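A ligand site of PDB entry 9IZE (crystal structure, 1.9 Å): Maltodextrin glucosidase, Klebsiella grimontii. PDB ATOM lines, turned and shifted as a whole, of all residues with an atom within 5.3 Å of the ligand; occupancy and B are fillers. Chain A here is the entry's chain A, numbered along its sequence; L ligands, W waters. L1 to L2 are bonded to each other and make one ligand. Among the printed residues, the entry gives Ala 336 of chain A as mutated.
An oxygen (O2) of LIG L1 is in hydrogen-bond range of the side-chain carboxylate (OD2) of Asp 448 (2.4 Å).
The side-chain carboxylate of Glu 373 lies within hydrogen-bond range of an oxygen (O1) of LIG L1 (2.4 Å).
An oxygen (O2) of LG2 L2 sits at hydrogen-bond distance from the backbone carbonyl oxygen of Asp 492, at 3.4 Å.
An oxygen (O4) of LG2 L2 sits at hydrogen-bond distance from the side-chain carboxylate of Asp 492 (2.5 Å).
The guanidinium group (NH2) of Arg 334 is in hydrogen-bond range of an oxygen (O2) of LIG L1, 2.9 Å away.
A ring nitrogen (NE2) of His 447 is in hydrogen-bond range of an oxygen (O2) of LIG L1.
A ring nitrogen (NE2) of His 251 sits at hydrogen-bond distance from an oxygen (O6) of LIG L1, at 3.0 Å.
An oxygen (O3) of LG2 L2 sits at hydrogen-bond distance from the guanidinium group (NH2) of Arg 496, 3.0 Å away.
An oxygen (O7) of LG2 L2 lies close to the side-chain hydroxyl (OH) of Tyr 295, 3.5 Å away.
A ring nitrogen (NE2) of His 447 lies within hydrogen-bond range of the side-chain carboxylate of Asp 448, at 3.3 Å.
The side-chain carboxylate (OD1) of Asp 448 lies within salt-bridge range of the guanidinium group (NH2) of Arg 496 (3.2 Å).
OD2 of Asp 492 is in salt-bridge range of NH2 of Arg 496, 3.1 Å away.
The guanidinium group of Arg 334 lies within hydrogen-bond range of the side-chain hydroxyl of Tyr 211 (3.5 Å).
O of His 447 sits at hydrogen-bond distance from NH2 of Arg 496, 2.8 Å away.
A ring nitrogen (NE2) of His 447 lies within hydrogen-bond range of the side-chain hydroxyl (OH) of Tyr 211 (2.9 Å).
ND1 of His 209 sits at hydrogen-bond distance from N of Tyr 211 (3.1 Å).
N of Trp 292 lies within hydrogen-bond range of O of Leu 298 (2.9 Å).
Merely in contact with the ligand: Tyr 211 (3.2 Å), Ala 336 (3.3 Å), Val 337 (3.4 Å), His 209 (3.5 Å), Trp 292 (3.7 Å) and Leu 298 (3.9 Å).
Hydrophobic or aromatic side chains that line the ligand: His 209, Tyr 211, His 251, Trp 292, Tyr 295, Leu 298, Ala 336, Val 337 and His 447.
14 residues have an atom within 4 Å of the ligand: His 209, Tyr 211, His 251, Trp 292, Tyr 295, Leu 298, Arg 334, Ala 336, Val 337, Glu 373, His 447, Asp 448, Asp 492 and Arg 496.
The nearest printed residue that does not touch the ligand is Gly 171 (4.3 Å).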
ATOM      1  N   PHE A 129      -7.916   6.179 -14.815  1.00  0.00           N
ATOM      2  CA  PHE A 129      -7.052   5.449 -15.741  1.00  0.00           C
ATOM      3  C   PHE A 129      -7.990   4.609 -16.609  1.00  0.00           C
ATOM      4  O   PHE A 129      -8.478   3.569 -16.153  1.00  0.00           O
ATOM      5  CB  PHE A 129      -6.052   4.592 -14.949  1.00  0.00           C
ATOM      6  CG  PHE A 129      -4.953   3.978 -15.777  1.00  0.00           C
ATOM      7  CD1 PHE A 129      -3.751   4.649 -15.981  1.00  0.00           C
ATOM      8  CD2 PHE A 129      -5.101   2.706 -16.301  1.00  0.00           C
ATOM      9  CE1 PHE A 129      -2.731   4.072 -16.721  1.00  0.00           C
ATOM     10  CE2 PHE A 129      -4.089   2.114 -17.040  1.00  0.00           C
ATOM     11  CZ  PHE A 129      -2.900   2.804 -17.251  1.00  0.00           C
ATOM     12  N   GLY A 170       3.311  -5.163 -18.193  1.00  0.00           N
ATOM     13  CA  GLY A 170       2.579  -4.154 -17.451  1.00  0.00           C
ATOM     14  C   GLY A 170       2.006  -3.059 -18.330  1.00  0.00           C
ATOM     15  O   GLY A 170       0.928  -2.531 -18.051  1.00  0.00           O
ATOM     16  N   GLY A 171       2.727  -2.687 -19.390  1.00  0.00           N
ATOM     17  CA  GLY A 171       2.303  -1.683 -20.337  1.00  0.00           C
ATOM     18  C   GLY A 171       1.502  -2.201 -21.513  1.00  0.00           C
ATOM     19  O   GLY A 171       1.141  -1.414 -22.393  1.00  0.00           O
ATOM     20  N   HIS A 209      -1.359   2.454 -20.996  1.00  0.00           N
ATOM     21  CA  HIS A 209      -1.377   3.762 -20.329  1.00  0.00           C
ATOM     22  C   HIS A 209      -1.419   4.906 -21.332  1.00  0.00           C
ATOM     23  O   HIS A 209      -1.919   5.995 -20.994  1.00  0.00           O
ATOM     24  CB  HIS A 209      -0.145   3.914 -19.434  1.00  0.00           C
ATOM     25  CG  HIS A 209       1.137   3.603 -20.125  1.00  0.00           C
ATOM     26  ND1 HIS A 209       1.726   4.452 -21.038  1.00  0.00           N
ATOM     27  CD2 HIS A 209       1.931   2.505 -20.070  1.00  0.00           C
ATOM     28  CE1 HIS A 209       2.834   3.910 -21.495  1.00  0.00           C
ATOM     29  NE2 HIS A 209       2.981   2.718 -20.929  1.00  0.00           N
ATOM     30  N   TYR A 211       0.838   6.928 -22.647  1.00  0.00           N
ATOM     31  CA  TYR A 211       1.785   8.049 -22.636  1.00  0.00           C
ATOM     32  C   TYR A 211       2.746   7.981 -23.818  1.00  0.00           C
ATOM     33  O   TYR A 211       3.541   8.913 -24.011  1.00  0.00           O
ATOM     34  CB  TYR A 211       2.539   8.075 -21.318  1.00  0.00           C
ATOM     35  CG  TYR A 211       1.692   8.562 -20.178  1.00  0.00           C
ATOM     36  CD1 TYR A 211       1.458   9.928 -19.997  1.00  0.00           C
ATOM     37  CD2 TYR A 211       1.096   7.675 -19.298  1.00  0.00           C
ATOM     38  CE1 TYR A 211       0.658  10.394 -18.951  1.00  0.00           C
ATOM     39  CE2 TYR A 211       0.287   8.127 -18.251  1.00  0.00           C
ATOM     40  CZ  TYR A 211       0.074   9.479 -18.084  1.00  0.00           C
ATOM     41  OH  TYR A 211      -0.705   9.927 -17.046  1.00  0.00           O
ATOM     42  N   VAL A 248       0.638  15.200 -22.982  1.00  0.00           N
ATOM     43  CA  VAL A 248       1.956  14.586 -22.923  1.00  0.00           C
ATOM     44  C   VAL A 248       2.826  15.199 -24.002  1.00  0.00           C
ATOM     45  O   VAL A 248       2.886  14.699 -25.138  1.00  0.00           O
ATOM     46  CB  VAL A 248       1.852  13.057 -23.050  1.00  0.00           C
ATOM     47  CG1 VAL A 248       3.162  12.383 -22.667  1.00  0.00           C
ATOM     48  CG2 VAL A 248       0.721  12.541 -22.172  1.00  0.00           C
ATOM     49  N   HIS A 251       7.490  14.526 -24.591  1.00  0.00           N
ATOM     50  CA  HIS A 251       7.913  13.467 -25.494  1.00  0.00           C
ATOM     51  C   HIS A 251       6.690  12.960 -26.231  1.00  0.00           C
ATOM     52  O   HIS A 251       5.556  13.148 -25.783  1.00  0.00           O
ATOM     53  CB  HIS A 251       8.574  12.335 -24.718  1.00  0.00           C
ATOM     54  CG  HIS A 251       7.730  11.778 -23.609  1.00  0.00           C
ATOM     55  ND1 HIS A 251       7.858  12.177 -22.301  1.00  0.00           N
ATOM     56  CD2 HIS A 251       6.747  10.845 -23.623  1.00  0.00           C
ATOM     57  CE1 HIS A 251       7.001  11.505 -21.546  1.00  0.00           C
ATOM     58  NE2 HIS A 251       6.309  10.695 -22.327  1.00  0.00           N
ATOM     59  N   TRP A 292      12.662   9.817 -22.596  1.00  0.00           N
ATOM     60  CA  TRP A 292      12.243  10.033 -21.211  1.00  0.00           C
ATOM     61  C   TRP A 292      12.919   8.994 -20.343  1.00  0.00           C
ATOM     62  O   TRP A 292      12.546   7.823 -20.333  1.00  0.00           O
ATOM     63  CB  TRP A 292      10.724   9.981 -21.063  1.00  0.00           C
ATOM     64  CG  TRP A 292      10.280  10.252 -19.652  1.00  0.00           C
ATOM     65  CD1 TRP A 292      10.218  11.478 -19.047  1.00  0.00           C
ATOM     66  CD2 TRP A 292       9.851   9.300 -18.673  1.00  0.00           C
ATOM     67  NE1 TRP A 292       9.767  11.342 -17.751  1.00  0.00           N
ATOM     68  CE2 TRP A 292       9.534  10.017 -17.498  1.00  0.00           C
ATOM     69  CE3 TRP A 292       9.699   7.908 -18.670  1.00  0.00           C
ATOM     70  CZ2 TRP A 292       9.076   9.394 -16.333  1.00  0.00           C
ATOM     71  CZ3 TRP A 292       9.240   7.283 -17.518  1.00  0.00           C
ATOM     72  CH2 TRP A 292       8.937   8.030 -16.361  1.00  0.00           C
ATOM     73  N   TYR A 295      13.694   5.411 -21.728  1.00  0.00           N
ATOM     74  CA  TYR A 295      12.687   4.554 -22.342  1.00  0.00           C
ATOM     75  C   TYR A 295      12.620   4.904 -23.824  1.00  0.00           C
ATOM     76  O   TYR A 295      12.148   5.992 -24.191  1.00  0.00           O
ATOM     77  CB  TYR A 295      11.344   4.715 -21.638  1.00  0.00           C
ATOM     78  CG  TYR A 295      11.335   4.137 -20.221  1.00  0.00           C
ATOM     79  CD1 TYR A 295      11.030   2.801 -19.991  1.00  0.00           C
ATOM     80  CD2 TYR A 295      11.649   4.928 -19.115  1.00  0.00           C
ATOM     81  CE1 TYR A 295      11.026   2.260 -18.705  1.00  0.00           C
ATOM     82  CE2 TYR A 295      11.655   4.395 -17.823  1.00  0.00           C
ATOM     83  CZ  TYR A 295      11.347   3.064 -17.629  1.00  0.00           C
ATOM     84  OH  TYR A 295      11.349   2.552 -16.346  1.00  0.00           O
ATOM     85  N   LEU A 298       9.707   6.519 -25.738  1.00  0.00           N
ATOM     86  CA  LEU A 298       9.284   7.875 -25.394  1.00  0.00           C
ATOM     87  C   LEU A 298      10.333   8.884 -25.837  1.00  0.00           C
ATOM     88  O   LEU A 298      11.025   9.489 -25.007  1.00  0.00           O
ATOM     89  CB  LEU A 298       9.001   7.973 -23.897  1.00  0.00           C
ATOM     90  CG  LEU A 298       7.991   6.946 -23.371  1.00  0.00           C
ATOM     91  CD1 LEU A 298       7.902   6.956 -21.853  1.00  0.00           C
ATOM     92  CD2 LEU A 298       6.610   7.176 -23.982  1.00  0.00           C
ATOM     93  N   ARG A 334      -3.721  18.438 -17.846  1.00  0.00           N
ATOM     94  CA  ARG A 334      -2.711  17.992 -16.897  1.00  0.00           C
ATOM     95  C   ARG A 334      -1.428  17.768 -17.700  1.00  0.00           C
ATOM     96  O   ARG A 334      -1.429  16.984 -18.657  1.00  0.00           O
ATOM     97  CB  ARG A 334      -3.180  16.727 -16.171  1.00  0.00           C
ATOM     98  CG  ARG A 334      -2.201  16.071 -15.185  1.00  0.00           C
ATOM     99  CD  ARG A 334      -1.203  15.144 -15.880  1.00  0.00           C
ATOM    100  NE  ARG A 334      -0.477  14.309 -14.936  1.00  0.00           N
ATOM    101  CZ  ARG A 334       0.379  13.353 -15.292  1.00  0.00           C
ATOM    102  NH1 ARG A 334       0.629  13.099 -16.571  1.00  0.00           N
ATOM    103  NH2 ARG A 334       0.987  12.645 -14.349  1.00  0.00           N
ATOM    104  N   ALA A 336       1.910  16.261 -18.393  1.00  0.00           N
ATOM    105  CA  ALA A 336       2.825  15.181 -18.049  1.00  0.00           C
ATOM    106  C   ALA A 336       4.271  15.662 -18.157  1.00  0.00           C
ATOM    107  O   ALA A 336       4.648  16.314 -19.135  1.00  0.00           O
ATOM    108  CB  ALA A 336       2.605  13.998 -18.979  1.00  0.00           C
ATOM    109  N   VAL A 337       5.080  15.314 -17.151  1.00  0.00           N
ATOM    110  CA  VAL A 337       6.519  15.599 -17.160  1.00  0.00           C
ATOM    111  C   VAL A 337       6.759  17.071 -17.473  1.00  0.00           C
ATOM    112  O   VAL A 337       7.634  17.422 -18.272  1.00  0.00           O
ATOM    113  CB  VAL A 337       7.250  14.683 -18.158  1.00  0.00           C
ATOM    114  CG1 VAL A 337       8.770  14.667 -17.868  1.00  0.00           C
ATOM    115  CG2 VAL A 337       6.689  13.282 -18.084  1.00  0.00           C
ATOM    116  N   GLU A 373       2.397  17.972 -13.716  1.00  0.00           N
ATOM    117  CA  GLU A 373       2.857  16.836 -12.919  1.00  0.00           C
ATOM    118  C   GLU A 373       4.176  17.202 -12.244  1.00  0.00           C
ATOM    119  O   GLU A 373       5.200  17.329 -12.918  1.00  0.00           O
ATOM    120  CB  GLU A 373       3.060  15.613 -13.804  1.00  0.00           C
ATOM    121  CG  GLU A 373       3.520  14.405 -13.002  1.00  0.00           C
ATOM    122  CD  GLU A 373       4.138  13.290 -13.829  1.00  0.00           C
ATOM    123  OE1 GLU A 373       4.565  13.539 -14.982  1.00  0.00           O
ATOM    124  OE2 GLU A 373       4.204  12.157 -13.304  1.00  0.00           O
ATOM    125  N   HIS A 447      -1.760   6.892 -10.290  1.00  0.00           N
ATOM    126  CA  HIS A 447      -1.376   5.772 -11.143  1.00  0.00           C
ATOM    127  C   HIS A 447       0.134   5.566 -11.182  1.00  0.00           C
ATOM    128  O   HIS A 447       0.614   4.615 -11.812  1.00  0.00           O
ATOM    129  CB  HIS A 447      -1.897   6.001 -12.551  1.00  0.00           C
ATOM    130  CG  HIS A 447      -1.270   7.161 -13.238  1.00  0.00           C
ATOM    131  ND1 HIS A 447      -1.305   8.436 -12.716  1.00  0.00           N
ATOM    132  CD2 HIS A 447      -0.550   7.249 -14.386  1.00  0.00           C
ATOM    133  CE1 HIS A 447      -0.655   9.263 -13.525  1.00  0.00           C
ATOM    134  NE2 HIS A 447      -0.187   8.560 -14.554  1.00  0.00           N
ATOM    135  N   ASP A 448       0.887   6.454 -10.531  1.00  0.00           N
ATOM    136  CA  ASP A 448       2.347   6.374 -10.489  1.00  0.00           C
ATOM    137  C   ASP A 448       2.872   6.110  -9.086  1.00  0.00           C
ATOM    138  O   ASP A 448       4.084   6.257  -8.851  1.00  0.00           O
ATOM    139  CB  ASP A 448       2.966   7.668 -11.042  1.00  0.00           C
ATOM    140  CG  ASP A 448       2.769   7.842 -12.546  1.00  0.00           C
ATOM    141  OD1 ASP A 448       2.703   6.826 -13.291  1.00  0.00           O
ATOM    142  OD2 ASP A 448       2.694   9.014 -12.995  1.00  0.00           O
ATOM    143  N   ASN A 491       3.021  -0.200  -6.186  1.00  0.00           N
ATOM    144  CA  ASN A 491       3.200   0.741  -7.276  1.00  0.00           C
ATOM    145  C   ASN A 491       3.025   0.054  -8.625  1.00  0.00           C
ATOM    146  O   ASN A 491       3.106  -1.178  -8.741  1.00  0.00           O
ATOM    147  CB  ASN A 491       4.577   1.401  -7.199  1.00  0.00           C
ATOM    148  CG  ASN A 491       4.707   2.572  -8.145  1.00  0.00           C
ATOM    149  OD1 ASN A 491       3.708   3.220  -8.475  1.00  0.00           O
ATOM    150  ND2 ASN A 491       5.920   2.852  -8.600  1.00  0.00           N
ATOM    151  N   ASP A 492       2.721   0.870  -9.639  1.00  0.00           N
ATOM    152  CA  ASP A 492       2.743   0.570 -11.062  1.00  0.00           C
ATOM    153  C   ASP A 492       3.609  -0.652 -11.345  1.00  0.00           C
ATOM    154  O   ASP A 492       4.834  -0.611 -11.125  1.00  0.00           O
ATOM    155  CB  ASP A 492       3.275   1.799 -11.818  1.00  0.00           C
ATOM    156  CG  ASP A 492       3.234   1.629 -13.317  1.00  0.00           C
ATOM    157  OD1 ASP A 492       2.601   0.680 -13.816  1.00  0.00           O
ATOM    158  OD2 ASP A 492       3.841   2.471 -14.010  1.00  0.00           O
ATOM    159  N   PRO A 493       3.035  -1.752 -11.866  1.00  0.00           N
ATOM    160  CA  PRO A 493       1.675  -1.895 -12.433  1.00  0.00           C
ATOM    161  C   PRO A 493       0.562  -2.166 -11.438  1.00  0.00           C
ATOM    162  O   PRO A 493      -0.615  -2.125 -11.823  1.00  0.00           O
ATOM    163  CB  PRO A 493       1.851  -3.097 -13.373  1.00  0.00           C
ATOM    164  CG  PRO A 493       2.833  -3.987 -12.621  1.00  0.00           C
ATOM    165  CD  PRO A 493       3.790  -3.020 -11.939  1.00  0.00           C
ATOM    166  N   ARG A 496      -3.016  -0.078 -10.512  1.00  0.00           N
ATOM    167  CA  ARG A 496      -3.980   0.174 -11.586  1.00  0.00           C
ATOM    168  C   ARG A 496      -4.964  -0.981 -11.741  1.00  0.00           C
ATOM    169  O   ARG A 496      -5.274  -1.414 -12.842  1.00  0.00           O
ATOM    170  CB  ARG A 496      -3.245   0.456 -12.889  1.00  0.00           C
ATOM    171  CG  ARG A 496      -2.220   1.587 -12.763  1.00  0.00           C
ATOM    172  CD  ARG A 496      -1.244   1.651 -13.927  1.00  0.00           C
ATOM    173  NE  ARG A 496      -0.293   2.753 -13.758  1.00  0.00           N
ATOM    174  CZ  ARG A 496       0.542   3.176 -14.702  1.00  0.00           C
ATOM    175  NH1 ARG A 496       0.598   2.593 -15.896  1.00  0.00           N
ATOM    176  NH2 ARG A 496       1.314   4.222 -14.453  1.00  0.00           N
HETATM  177  C1  LIG L   1       3.607  10.685 -17.158  1.00  0.00           C
HETATM  178  C2  LIG L   1       2.802   9.651 -16.354  1.00  0.00           C
HETATM  179  C3  LIG L   1       3.529   8.382 -16.141  1.00  0.00           C
HETATM  180  C4  LIG L   1       4.284   7.991 -17.381  1.00  0.00           C
HETATM  181  C5  LIG L   1       5.448   8.965 -17.566  1.00  0.00           C
HETATM  182  C6  LIG L   1       6.165   8.822 -18.890  1.00  0.00           C
HETATM  183  O1  LIG L   1       3.651  11.932 -16.583  1.00  0.00           O
HETATM  184  O2  LIG L   1       2.274  10.159 -15.109  1.00  0.00           O
HETATM  185  O3  LIG L   1       2.478   7.411 -15.786  1.00  0.00           O
HETATM  186  O4  LIG L   1       4.755   6.633 -17.238  1.00  0.00           O
HETATM  187  O5  LIG L   1       5.008  10.352 -17.529  1.00  0.00           O
HETATM  188  O6  LIG L   1       5.259   9.206 -19.913  1.00  0.00           O
HETATM  189  O1  LG2 L   2       5.422   5.387 -19.103  1.00  0.00           O
HETATM  190  C1  LG2 L   2       3.602   4.643 -17.838  1.00  0.00           C
HETATM  191  C2  LG2 L   2       4.421   4.004 -16.807  1.00  0.00           C
HETATM  192  C3  LG2 L   2       7.241   0.372 -17.843  1.00  0.00           C
HETATM  193  C4  LG2 L   2       8.020   0.969 -13.475  1.00  0.00           C
HETATM  194  C5  LG2 L   2       8.006   1.124 -14.990  1.00  0.00           C
HETATM  195  C6  LG2 L   2       6.641   1.588 -15.667  1.00  0.00           C
HETATM  196  C7  LG2 L   2       6.951   1.830 -17.032  1.00  0.00           C
HETATM  197  C8  LG2 L   2       5.837   3.772 -17.199  1.00  0.00           C
HETATM  198  C9  LG2 L   2       6.450   4.753 -18.229  1.00  0.00           C
HETATM  199  C10 LG2 L   2       7.482   4.210 -19.157  1.00  0.00           C
HETATM  200  C11 LG2 L   2       4.292   5.894 -18.337  1.00  0.00           C
HETATM  201  C12 LG2 L   2       7.977  -0.438 -17.122  1.00  0.00           C
HETATM  202  C13 LG2 L   2       8.872   0.403 -15.881  1.00  0.00           C
HETATM  203  N1  LG2 L   2       5.804   2.363 -17.637  1.00  0.00           N
HETATM  204  O2  LG2 L   2       6.723   1.414 -13.147  1.00  0.00           O
HETATM  205  O3  LG2 L   2       2.414   5.001 -17.164  1.00  0.00           O
HETATM  206  O4  LG2 L   2       3.747   2.737 -16.529  1.00  0.00           O
HETATM  207  O5  LG2 L   2       5.877  -0.042 -18.136  1.00  0.00           O
HETATM  208  O6  LG2 L   2       8.915  -1.045 -18.061  1.00  0.00           O
HETATM  209  O7  LG2 L   2       9.772  -0.311 -15.106  1.00  0.00           O
HETATM  210  O   HOH W   1      11.377  -2.060 -19.473  1.00  0.00           O
HETATM  211  O   HOH W   2       6.472   6.077 -14.610  1.00  0.00           O
